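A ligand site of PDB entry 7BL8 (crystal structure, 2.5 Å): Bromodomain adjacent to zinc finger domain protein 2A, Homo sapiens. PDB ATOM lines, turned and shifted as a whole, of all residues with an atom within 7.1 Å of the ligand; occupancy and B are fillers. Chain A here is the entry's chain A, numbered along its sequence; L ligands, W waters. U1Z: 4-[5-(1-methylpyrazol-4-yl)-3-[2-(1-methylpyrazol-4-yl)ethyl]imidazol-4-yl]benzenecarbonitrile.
N27 of the ligand lies within hydrogen-bond range of N of Asn 30, at 2.8 Å. The backbone NH (N) of Glu 27 sits at hydrogen-bond distance from a nitrogen (N23) of the ligand (2.9 Å). N of Leu 26 is in hydrogen-bond range of N23 of the ligand (3.1 Å). A nitrogen (N15) of the ligand lies within hydrogen-bond range of the side-chain amide nitrogen (ND2) of Asn 80.
Water W5 bridges a nitrogen (N09) of the ligand (2.9 Å) and the side-chain amide oxygen (OD1) of Asn 80 (3.3 Å). Water W3 lies within hydrogen-bond range of OH of Tyr 37, N15 of the ligand, O of Asn 75 and N of Cys 76. Water W2 bridges a nitrogen (N23) of the ligand (3.1 Å) and the backbone carbonyl oxygen of Trp 23 (3.3 Å).
The backbone NH (N) of Arg 32 lies within hydrogen-bond range of the side-chain amide oxygen (OD1) of Asn 30. The side-chain amide nitrogen of Asn 80 is in hydrogen-bond range of the backbone carbonyl oxygen of Cys 76 (3.1 Å). The backbone carbonyl oxygen (O) of Val 86 lies within hydrogen-bond range of the side-chain sulfur (SG) of Cys 76 (3.7 Å).
A nitrogen (N23) of the ligand sits close to the backbone carbonyl oxygen (O) of Trp 23 (3.5 Å). Pro 24 touches the ligand (O to C14, 3.3 Å). CE1 of Phe 25 touches C14 of the ligand, at 3.5 Å. Pro 28 touches the ligand (O to C01, 3.4 Å). Val 29 touches the ligand. CB of Leu 33 touches C26 of the ligand, at 3.8 Å. Val 34 touches the ligand. CG1 of Val 86 touches N13 of the ligand, 3.6 Å away. Hydrophobic or aromatic side chains within 4 Å of the ligand: Pro 24, Phe 25, Leu 26, Val 29, Leu 33, Val 34 and Val 86.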
ATOM      1  N   ALA A  22      -2.478 -16.302  35.780  1.00  0.00           N
ATOM      2  CA  ALA A  22      -3.214 -17.431  35.232  1.00  0.00           C
ATOM      3  C   ALA A  22      -4.715 -17.289  35.379  1.00  0.00           C
ATOM      4  O   ALA A  22      -5.449 -18.172  34.925  1.00  0.00           O
ATOM      5  CB  ALA A  22      -2.761 -18.735  35.890  1.00  0.00           C
ATOM      6  N   TRP A  23      -5.200 -16.188  35.968  1.00  0.00           N
ATOM      7  CA  TRP A  23      -6.626 -16.099  36.250  1.00  0.00           C
ATOM      8  C   TRP A  23      -7.556 -16.211  35.030  1.00  0.00           C
ATOM      9  O   TRP A  23      -8.722 -16.586  35.240  1.00  0.00           O
ATOM     10  CB  TRP A  23      -6.918 -14.819  37.042  1.00  0.00           C
ATOM     11  CG  TRP A  23      -6.577 -13.580  36.306  1.00  0.00           C
ATOM     12  CD1 TRP A  23      -5.436 -12.878  36.417  1.00  0.00           C
ATOM     13  CD2 TRP A  23      -7.388 -12.883  35.352  1.00  0.00           C
ATOM     14  NE1 TRP A  23      -5.455 -11.786  35.580  1.00  0.00           N
ATOM     15  CE2 TRP A  23      -6.650 -11.771  34.911  1.00  0.00           C
ATOM     16  CE3 TRP A  23      -8.655 -13.120  34.802  1.00  0.00           C
ATOM     17  CZ2 TRP A  23      -7.137 -10.869  33.957  1.00  0.00           C
ATOM     18  CZ3 TRP A  23      -9.147 -12.218  33.857  1.00  0.00           C
ATOM     19  CH2 TRP A  23      -8.386 -11.107  33.441  1.00  0.00           C
ATOM     20  N   PRO A  24      -7.150 -15.914  33.789  1.00  0.00           N
ATOM     21  CA  PRO A  24      -8.064 -16.145  32.658  1.00  0.00           C
ATOM     22  C   PRO A  24      -8.070 -17.554  32.111  1.00  0.00           C
ATOM     23  O   PRO A  24      -8.830 -17.825  31.183  1.00  0.00           O
ATOM     24  CB  PRO A  24      -7.555 -15.164  31.580  1.00  0.00           C
ATOM     25  CG  PRO A  24      -6.553 -14.333  32.234  1.00  0.00           C
ATOM     26  CD  PRO A  24      -5.989 -15.149  33.335  1.00  0.00           C
ATOM     27  N   PHE A  25      -7.255 -18.462  32.642  1.00  0.00           N
ATOM     28  CA  PHE A  25      -7.049 -19.772  32.020  1.00  0.00           C
ATOM     29  C   PHE A  25      -7.374 -20.924  32.948  1.00  0.00           C
ATOM     30  O   PHE A  25      -7.064 -22.076  32.616  1.00  0.00           O
ATOM     31  CB  PHE A  25      -5.604 -19.888  31.530  1.00  0.00           C
ATOM     32  CG  PHE A  25      -5.180 -18.734  30.704  1.00  0.00           C
ATOM     33  CD1 PHE A  25      -5.752 -18.518  29.470  1.00  0.00           C
ATOM     34  CD2 PHE A  25      -4.268 -17.796  31.191  1.00  0.00           C
ATOM     35  CE1 PHE A  25      -5.391 -17.415  28.700  1.00  0.00           C
ATOM     36  CE2 PHE A  25      -3.892 -16.697  30.441  1.00  0.00           C
ATOM     37  CZ  PHE A  25      -4.457 -16.503  29.188  1.00  0.00           C
ATOM     38  N   LEU A  26      -8.000 -20.677  34.100  1.00  0.00           N
ATOM     39  CA  LEU A  26      -8.164 -21.759  35.062  1.00  0.00           C
ATOM     40  C   LEU A  26      -9.315 -22.692  34.693  1.00  0.00           C
ATOM     41  O   LEU A  26      -9.214 -23.899  34.909  1.00  0.00           O
ATOM     42  CB  LEU A  26      -8.342 -21.190  36.470  1.00  0.00           C
ATOM     43  CG  LEU A  26      -7.094 -20.452  36.964  1.00  0.00           C
ATOM     44  CD1 LEU A  26      -7.348 -19.850  38.316  1.00  0.00           C
ATOM     45  CD2 LEU A  26      -5.890 -21.392  37.003  1.00  0.00           C
ATOM     46  N   GLU A  27     -10.378 -22.166  34.101  1.00  0.00           N
ATOM     47  CA  GLU A  27     -11.479 -22.984  33.633  1.00  0.00           C
ATOM     48  C   GLU A  27     -11.824 -22.576  32.218  1.00  0.00           C
ATOM     49  O   GLU A  27     -11.364 -21.527  31.734  1.00  0.00           O
ATOM     50  CB  GLU A  27     -12.702 -22.852  34.571  1.00  0.00           C
ATOM     51  CG  GLU A  27     -13.356 -21.483  34.627  1.00  0.00           C
ATOM     52  CD  GLU A  27     -14.267 -21.337  35.835  1.00  0.00           C
ATOM     53  OE1 GLU A  27     -15.001 -22.300  36.152  1.00  0.00           O
ATOM     54  OE2 GLU A  27     -14.230 -20.268  36.503  1.00  0.00           O
ATOM     55  N   PRO A  28     -12.571 -23.413  31.480  1.00  0.00           N
ATOM     56  CA  PRO A  28     -12.907 -23.071  30.093  1.00  0.00           C
ATOM     57  C   PRO A  28     -13.640 -21.750  29.978  1.00  0.00           C
ATOM     58  O   PRO A  28     -14.389 -21.348  30.864  1.00  0.00           O
ATOM     59  CB  PRO A  28     -13.792 -24.247  29.644  1.00  0.00           C
ATOM     60  CG  PRO A  28     -13.310 -25.388  30.422  1.00  0.00           C
ATOM     61  CD  PRO A  28     -12.927 -24.806  31.792  1.00  0.00           C
ATOM     62  N   VAL A  29     -13.414 -21.063  28.865  1.00  0.00           N
ATOM     63  CA  VAL A  29     -14.187 -19.873  28.589  1.00  0.00           C
ATOM     64  C   VAL A  29     -15.648 -20.275  28.401  1.00  0.00           C
ATOM     65  O   VAL A  29     -15.966 -21.195  27.642  1.00  0.00           O
ATOM     66  CB  VAL A  29     -13.662 -19.144  27.347  1.00  0.00           C
ATOM     67  CG1 VAL A  29     -14.691 -18.141  26.856  1.00  0.00           C
ATOM     68  CG2 VAL A  29     -12.379 -18.443  27.676  1.00  0.00           C
ATOM     69  N   ASN A  30     -16.514 -19.605  29.129  1.00  0.00           N
ATOM     70  CA  ASN A  30     -17.934 -19.908  29.102  1.00  0.00           C
ATOM     71  C   ASN A  30     -18.571 -19.035  28.028  1.00  0.00           C
ATOM     72  O   ASN A  30     -18.804 -17.845  28.266  1.00  0.00           O
ATOM     73  CB  ASN A  30     -18.547 -19.686  30.480  1.00  0.00           C
ATOM     74  CG  ASN A  30     -20.049 -19.919  30.510  1.00  0.00           C
ATOM     75  OD1 ASN A  30     -20.698 -20.061  29.473  1.00  0.00           O
ATOM     76  ND2 ASN A  30     -20.627 -19.933  31.723  1.00  0.00           N
ATOM     77  N   PRO A  31     -18.878 -19.597  26.851  1.00  0.00           N
ATOM     78  CA  PRO A  31     -19.333 -18.742  25.743  1.00  0.00           C
ATOM     79  C   PRO A  31     -20.636 -18.031  26.026  1.00  0.00           C
ATOM     80  O   PRO A  31     -20.876 -16.967  25.466  1.00  0.00           O
ATOM     81  CB  PRO A  31     -19.462 -19.736  24.574  1.00  0.00           C
ATOM     82  CG  PRO A  31     -19.671 -21.068  25.223  1.00  0.00           C
ATOM     83  CD  PRO A  31     -18.987 -21.036  26.567  1.00  0.00           C
ATOM     84  N   ARG A  32     -21.470 -18.564  26.920  1.00  0.00           N
ATOM     85  CA  ARG A  32     -22.660 -17.830  27.349  1.00  0.00           C
ATOM     86  C   ARG A  32     -22.314 -16.437  27.860  1.00  0.00           C
ATOM     87  O   ARG A  32     -23.135 -15.526  27.762  1.00  0.00           O
ATOM     88  CB  ARG A  32     -23.393 -18.609  28.437  1.00  0.00           C
ATOM     89  CG  ARG A  32     -24.167 -19.830  27.971  1.00  0.00           C
ATOM     90  CD  ARG A  32     -24.686 -20.606  29.169  1.00  0.00           C
ATOM     91  NE  ARG A  32     -25.336 -21.848  28.819  1.00  0.00           N
ATOM     92  CZ  ARG A  32     -25.738 -22.756  29.705  1.00  0.00           C
ATOM     93  NH1 ARG A  32     -25.553 -22.554  31.008  1.00  0.00           N
ATOM     94  NH2 ARG A  32     -26.307 -23.869  29.298  1.00  0.00           N
ATOM     95  N   LEU A  33     -21.132 -16.262  28.429  1.00  0.00           N
ATOM     96  CA  LEU A  33     -20.780 -15.022  29.092  1.00  0.00           C
ATOM     97  C   LEU A  33     -19.995 -14.072  28.206  1.00  0.00           C
ATOM     98  O   LEU A  33     -19.718 -12.946  28.608  1.00  0.00           O
ATOM     99  CB  LEU A  33     -20.001 -15.320  30.375  1.00  0.00           C
ATOM    100  CG  LEU A  33     -20.780 -16.130  31.414  1.00  0.00           C
ATOM    101  CD1 LEU A  33     -19.866 -16.734  32.508  1.00  0.00           C
ATOM    102  CD2 LEU A  33     -21.885 -15.291  32.030  1.00  0.00           C
ATOM    103  N   VAL A  34     -19.625 -14.492  27.001  1.00  0.00           N
ATOM    104  CA  VAL A  34     -18.649 -13.781  26.189  1.00  0.00           C
ATOM    105  C   VAL A  34     -19.134 -13.764  24.739  1.00  0.00           C
ATOM    106  O   VAL A  34     -19.109 -14.786  24.060  1.00  0.00           O
ATOM    107  CB  VAL A  34     -17.255 -14.418  26.291  1.00  0.00           C
ATOM    108  CG1 VAL A  34     -16.280 -13.681  25.443  1.00  0.00           C
ATOM    109  CG2 VAL A  34     -16.765 -14.404  27.732  1.00  0.00           C
ATOM    110  N   TYR A  37     -17.484 -15.748  21.255  1.00  0.00           N
ATOM    111  CA  TYR A  37     -16.431 -16.726  21.519  1.00  0.00           C
ATOM    112  C   TYR A  37     -16.708 -18.046  20.818  1.00  0.00           C
ATOM    113  O   TYR A  37     -15.782 -18.694  20.331  1.00  0.00           O
ATOM    114  CB  TYR A  37     -16.267 -16.950  23.027  1.00  0.00           C
ATOM    115  CG  TYR A  37     -14.927 -17.600  23.340  1.00  0.00           C
ATOM    116  CD1 TYR A  37     -13.771 -16.832  23.447  1.00  0.00           C
ATOM    117  CD2 TYR A  37     -14.817 -18.975  23.480  1.00  0.00           C
ATOM    118  CE1 TYR A  37     -12.545 -17.417  23.707  1.00  0.00           C
ATOM    119  CE2 TYR A  37     -13.597 -19.572  23.736  1.00  0.00           C
ATOM    120  CZ  TYR A  37     -12.465 -18.801  23.841  1.00  0.00           C
ATOM    121  OH  TYR A  37     -11.266 -19.405  24.096  1.00  0.00           O
ATOM    122  N   MET A  45      -9.174 -24.345  24.701  1.00  0.00           N
ATOM    123  CA  MET A  45      -8.270 -25.083  25.559  1.00  0.00           C
ATOM    124  C   MET A  45      -7.983 -24.208  26.761  1.00  0.00           C
ATOM    125  O   MET A  45      -8.017 -22.973  26.663  1.00  0.00           O
ATOM    126  CB  MET A  45      -6.987 -25.483  24.816  1.00  0.00           C
ATOM    127  CG  MET A  45      -6.038 -26.354  25.619  1.00  0.00           C
ATOM    128  SD  MET A  45      -6.781 -27.873  26.286  1.00  0.00           S
ATOM    129  CE  MET A  45      -7.322 -28.686  24.791  1.00  0.00           C
ATOM    130  N   ASP A  46      -7.752 -24.836  27.903  1.00  0.00           N
ATOM    131  CA  ASP A  46      -7.462 -24.123  29.140  1.00  0.00           C
ATOM    132  C   ASP A  46      -6.708 -25.059  30.073  1.00  0.00           C
ATOM    133  O   ASP A  46      -6.483 -26.229  29.773  1.00  0.00           O
ATOM    134  CB  ASP A  46      -8.748 -23.583  29.778  1.00  0.00           C
ATOM    135  CG  ASP A  46      -9.509 -24.665  30.516  1.00  0.00           C
ATOM    136  OD1 ASP A  46     -10.297 -25.385  29.859  1.00  0.00           O
ATOM    137  OD2 ASP A  46      -9.319 -24.798  31.752  1.00  0.00           O
ATOM    138  N   VAL A  72      -3.742 -22.634  23.989  1.00  0.00           N
ATOM    139  CA  VAL A  72      -4.349 -21.702  24.922  1.00  0.00           C
ATOM    140  C   VAL A  72      -4.001 -20.257  24.548  1.00  0.00           C
ATOM    141  O   VAL A  72      -4.864 -19.375  24.542  1.00  0.00           O
ATOM    142  CB  VAL A  72      -3.945 -22.025  26.371  1.00  0.00           C
ATOM    143  CG1 VAL A  72      -4.482 -20.968  27.311  1.00  0.00           C
ATOM    144  CG2 VAL A  72      -4.480 -23.377  26.800  1.00  0.00           C
ATOM    145  N   ASN A  75      -5.446 -18.994  21.082  1.00  0.00           N
ATOM    146  CA  ASN A  75      -6.863 -18.645  21.266  1.00  0.00           C
ATOM    147  C   ASN A  75      -6.988 -17.283  21.945  1.00  0.00           C
ATOM    148  O   ASN A  75      -7.780 -16.436  21.519  1.00  0.00           O
ATOM    149  CB  ASN A  75      -7.589 -19.741  22.058  1.00  0.00           C
ATOM    150  CG  ASN A  75      -7.882 -21.021  21.232  1.00  0.00           C
ATOM    151  OD1 ASN A  75      -7.976 -20.997  20.005  1.00  0.00           O
ATOM    152  ND2 ASN A  75      -8.047 -22.135  21.919  1.00  0.00           N
ATOM    153  N   CYS A  76      -6.149 -17.039  22.965  1.00  0.00           N
ATOM    154  CA  CYS A  76      -6.184 -15.770  23.695  1.00  0.00           C
ATOM    155  C   CYS A  76      -5.822 -14.590  22.811  1.00  0.00           C
ATOM    156  O   CYS A  76      -6.495 -13.545  22.833  1.00  0.00           O
ATOM    157  CB  CYS A  76      -5.254 -15.838  24.904  1.00  0.00           C
ATOM    158  SG  CYS A  76      -5.285 -14.360  25.959  1.00  0.00           S
ATOM    159  N   PHE A  79      -8.753 -14.030  20.303  1.00  0.00           N
ATOM    160  CA  PHE A  79      -9.993 -13.420  20.773  1.00  0.00           C
ATOM    161  C   PHE A  79      -9.785 -12.087  21.481  1.00  0.00           C
ATOM    162  O   PHE A  79     -10.658 -11.210  21.389  1.00  0.00           O
ATOM    163  CB  PHE A  79     -10.753 -14.381  21.684  1.00  0.00           C
ATOM    164  CG  PHE A  79     -12.153 -13.937  21.970  1.00  0.00           C
ATOM    165  CD1 PHE A  79     -13.169 -14.213  21.069  1.00  0.00           C
ATOM    166  CD2 PHE A  79     -12.455 -13.223  23.122  1.00  0.00           C
ATOM    167  CE1 PHE A  79     -14.469 -13.789  21.319  1.00  0.00           C
ATOM    168  CE2 PHE A  79     -13.747 -12.796  23.377  1.00  0.00           C
ATOM    169  CZ  PHE A  79     -14.753 -13.091  22.471  1.00  0.00           C
ATOM    170  N   ASN A  80      -8.695 -11.890  22.217  1.00  0.00           N
ATOM    171  CA  ASN A  80      -8.568 -10.697  23.051  1.00  0.00           C
ATOM    172  C   ASN A  80      -7.530  -9.730  22.494  1.00  0.00           C
ATOM    173  O   ASN A  80      -6.467 -10.139  22.016  1.00  0.00           O
ATOM    174  CB  ASN A  80      -8.217 -11.080  24.481  1.00  0.00           C
ATOM    175  CG  ASN A  80      -9.168 -12.108  25.031  1.00  0.00           C
ATOM    176  OD1 ASN A  80     -10.203 -11.760  25.605  1.00  0.00           O
ATOM    177  ND2 ASN A  80      -8.840 -13.391  24.835  1.00  0.00           N
ATOM    178  N   VAL A  86      -7.505  -9.512  29.642  1.00  0.00           N
ATOM    179  CA  VAL A  86      -7.199 -10.901  29.342  1.00  0.00           C
ATOM    180  C   VAL A  86      -5.974 -10.964  28.440  1.00  0.00           C
ATOM    181  O   VAL A  86      -5.077 -11.795  28.649  1.00  0.00           O
ATOM    182  CB  VAL A  86      -8.416 -11.620  28.716  1.00  0.00           C
ATOM    183  CG1 VAL A  86      -8.065 -13.014  28.234  1.00  0.00           C
ATOM    184  CG2 VAL A  86      -9.571 -11.688  29.727  1.00  0.00           C
HETATM  185  C01 U1Z L   1     -15.339 -18.907  32.998  1.00  0.00           C
HETATM  186  C03 U1Z L   1     -15.732 -16.470  32.906  1.00  0.00           C
HETATM  187  C04 U1Z L   1     -16.113 -15.563  31.932  1.00  0.00           C
HETATM  188  C05 U1Z L   1     -16.307 -14.060  32.090  1.00  0.00           C
HETATM  189  C06 U1Z L   1     -14.994 -13.303  32.183  1.00  0.00           C
HETATM  190  C08 U1Z L   1     -14.311 -12.738  29.880  1.00  0.00           C
HETATM  191  C10 U1Z L   1     -12.739 -14.169  29.483  1.00  0.00           C
HETATM  192  C11 U1Z L   1     -11.647 -14.892  28.688  1.00  0.00           C
HETATM  193  C12 U1Z L   1     -10.610 -15.701  29.127  1.00  0.00           C
HETATM  194  C14 U1Z L   1      -8.778 -16.961  28.015  1.00  0.00           C
HETATM  195  C16 U1Z L   1     -11.550 -14.818  27.305  1.00  0.00           C
HETATM  196  C17 U1Z L   1     -13.223 -14.377  30.761  1.00  0.00           C
HETATM  197  C18 U1Z L   1     -12.682 -15.466  31.699  1.00  0.00           C
HETATM  198  C19 U1Z L   1     -12.718 -16.800  31.284  1.00  0.00           C
HETATM  199  C20 U1Z L   1     -12.199 -17.799  32.096  1.00  0.00           C
HETATM  200  C21 U1Z L   1     -11.646 -17.474  33.332  1.00  0.00           C
HETATM  201  C22 U1Z L   1     -11.089 -18.579  34.210  1.00  0.00           C
HETATM  202  C24 U1Z L   1     -11.609 -16.159  33.758  1.00  0.00           C
HETATM  203  C25 U1Z L   1     -12.121 -15.150  32.928  1.00  0.00           C
HETATM  204  C26 U1Z L   1     -16.293 -16.278  30.758  1.00  0.00           C
HETATM  205  N02 U1Z L   1     -15.697 -17.661  32.337  1.00  0.00           N
HETATM  206  N07 U1Z L   1     -14.185 -13.486  30.986  1.00  0.00           N
HETATM  207  N09 U1Z L   1     -13.424 -13.179  28.969  1.00  0.00           N
HETATM  208  N13 U1Z L   1      -9.948 -16.085  28.042  1.00  0.00           N
HETATM  209  N15 U1Z L   1     -10.525 -15.563  26.897  1.00  0.00           N
HETATM  210  N23 U1Z L   1     -10.680 -19.414  34.855  1.00  0.00           N
HETATM  211  N27 U1Z L   1     -16.043 -17.554  31.012  1.00  0.00           N
HETATM  212  O   HOH W   1      -8.428 -20.319  27.459  1.00  0.00           O
HETATM  213  O   HOH W   2     -10.688 -17.780  37.547  1.00  0.00           O
HETATM  214  O   HOH W   3      -9.269 -17.198  24.536  1.00  0.00           O
HETATM  215  O   HOH W   4      -7.173 -18.799  25.680  1.00  0.00           O
HETATM  216  O   HOH W   5     -13.364 -11.494  26.614  1.00  0.00           O
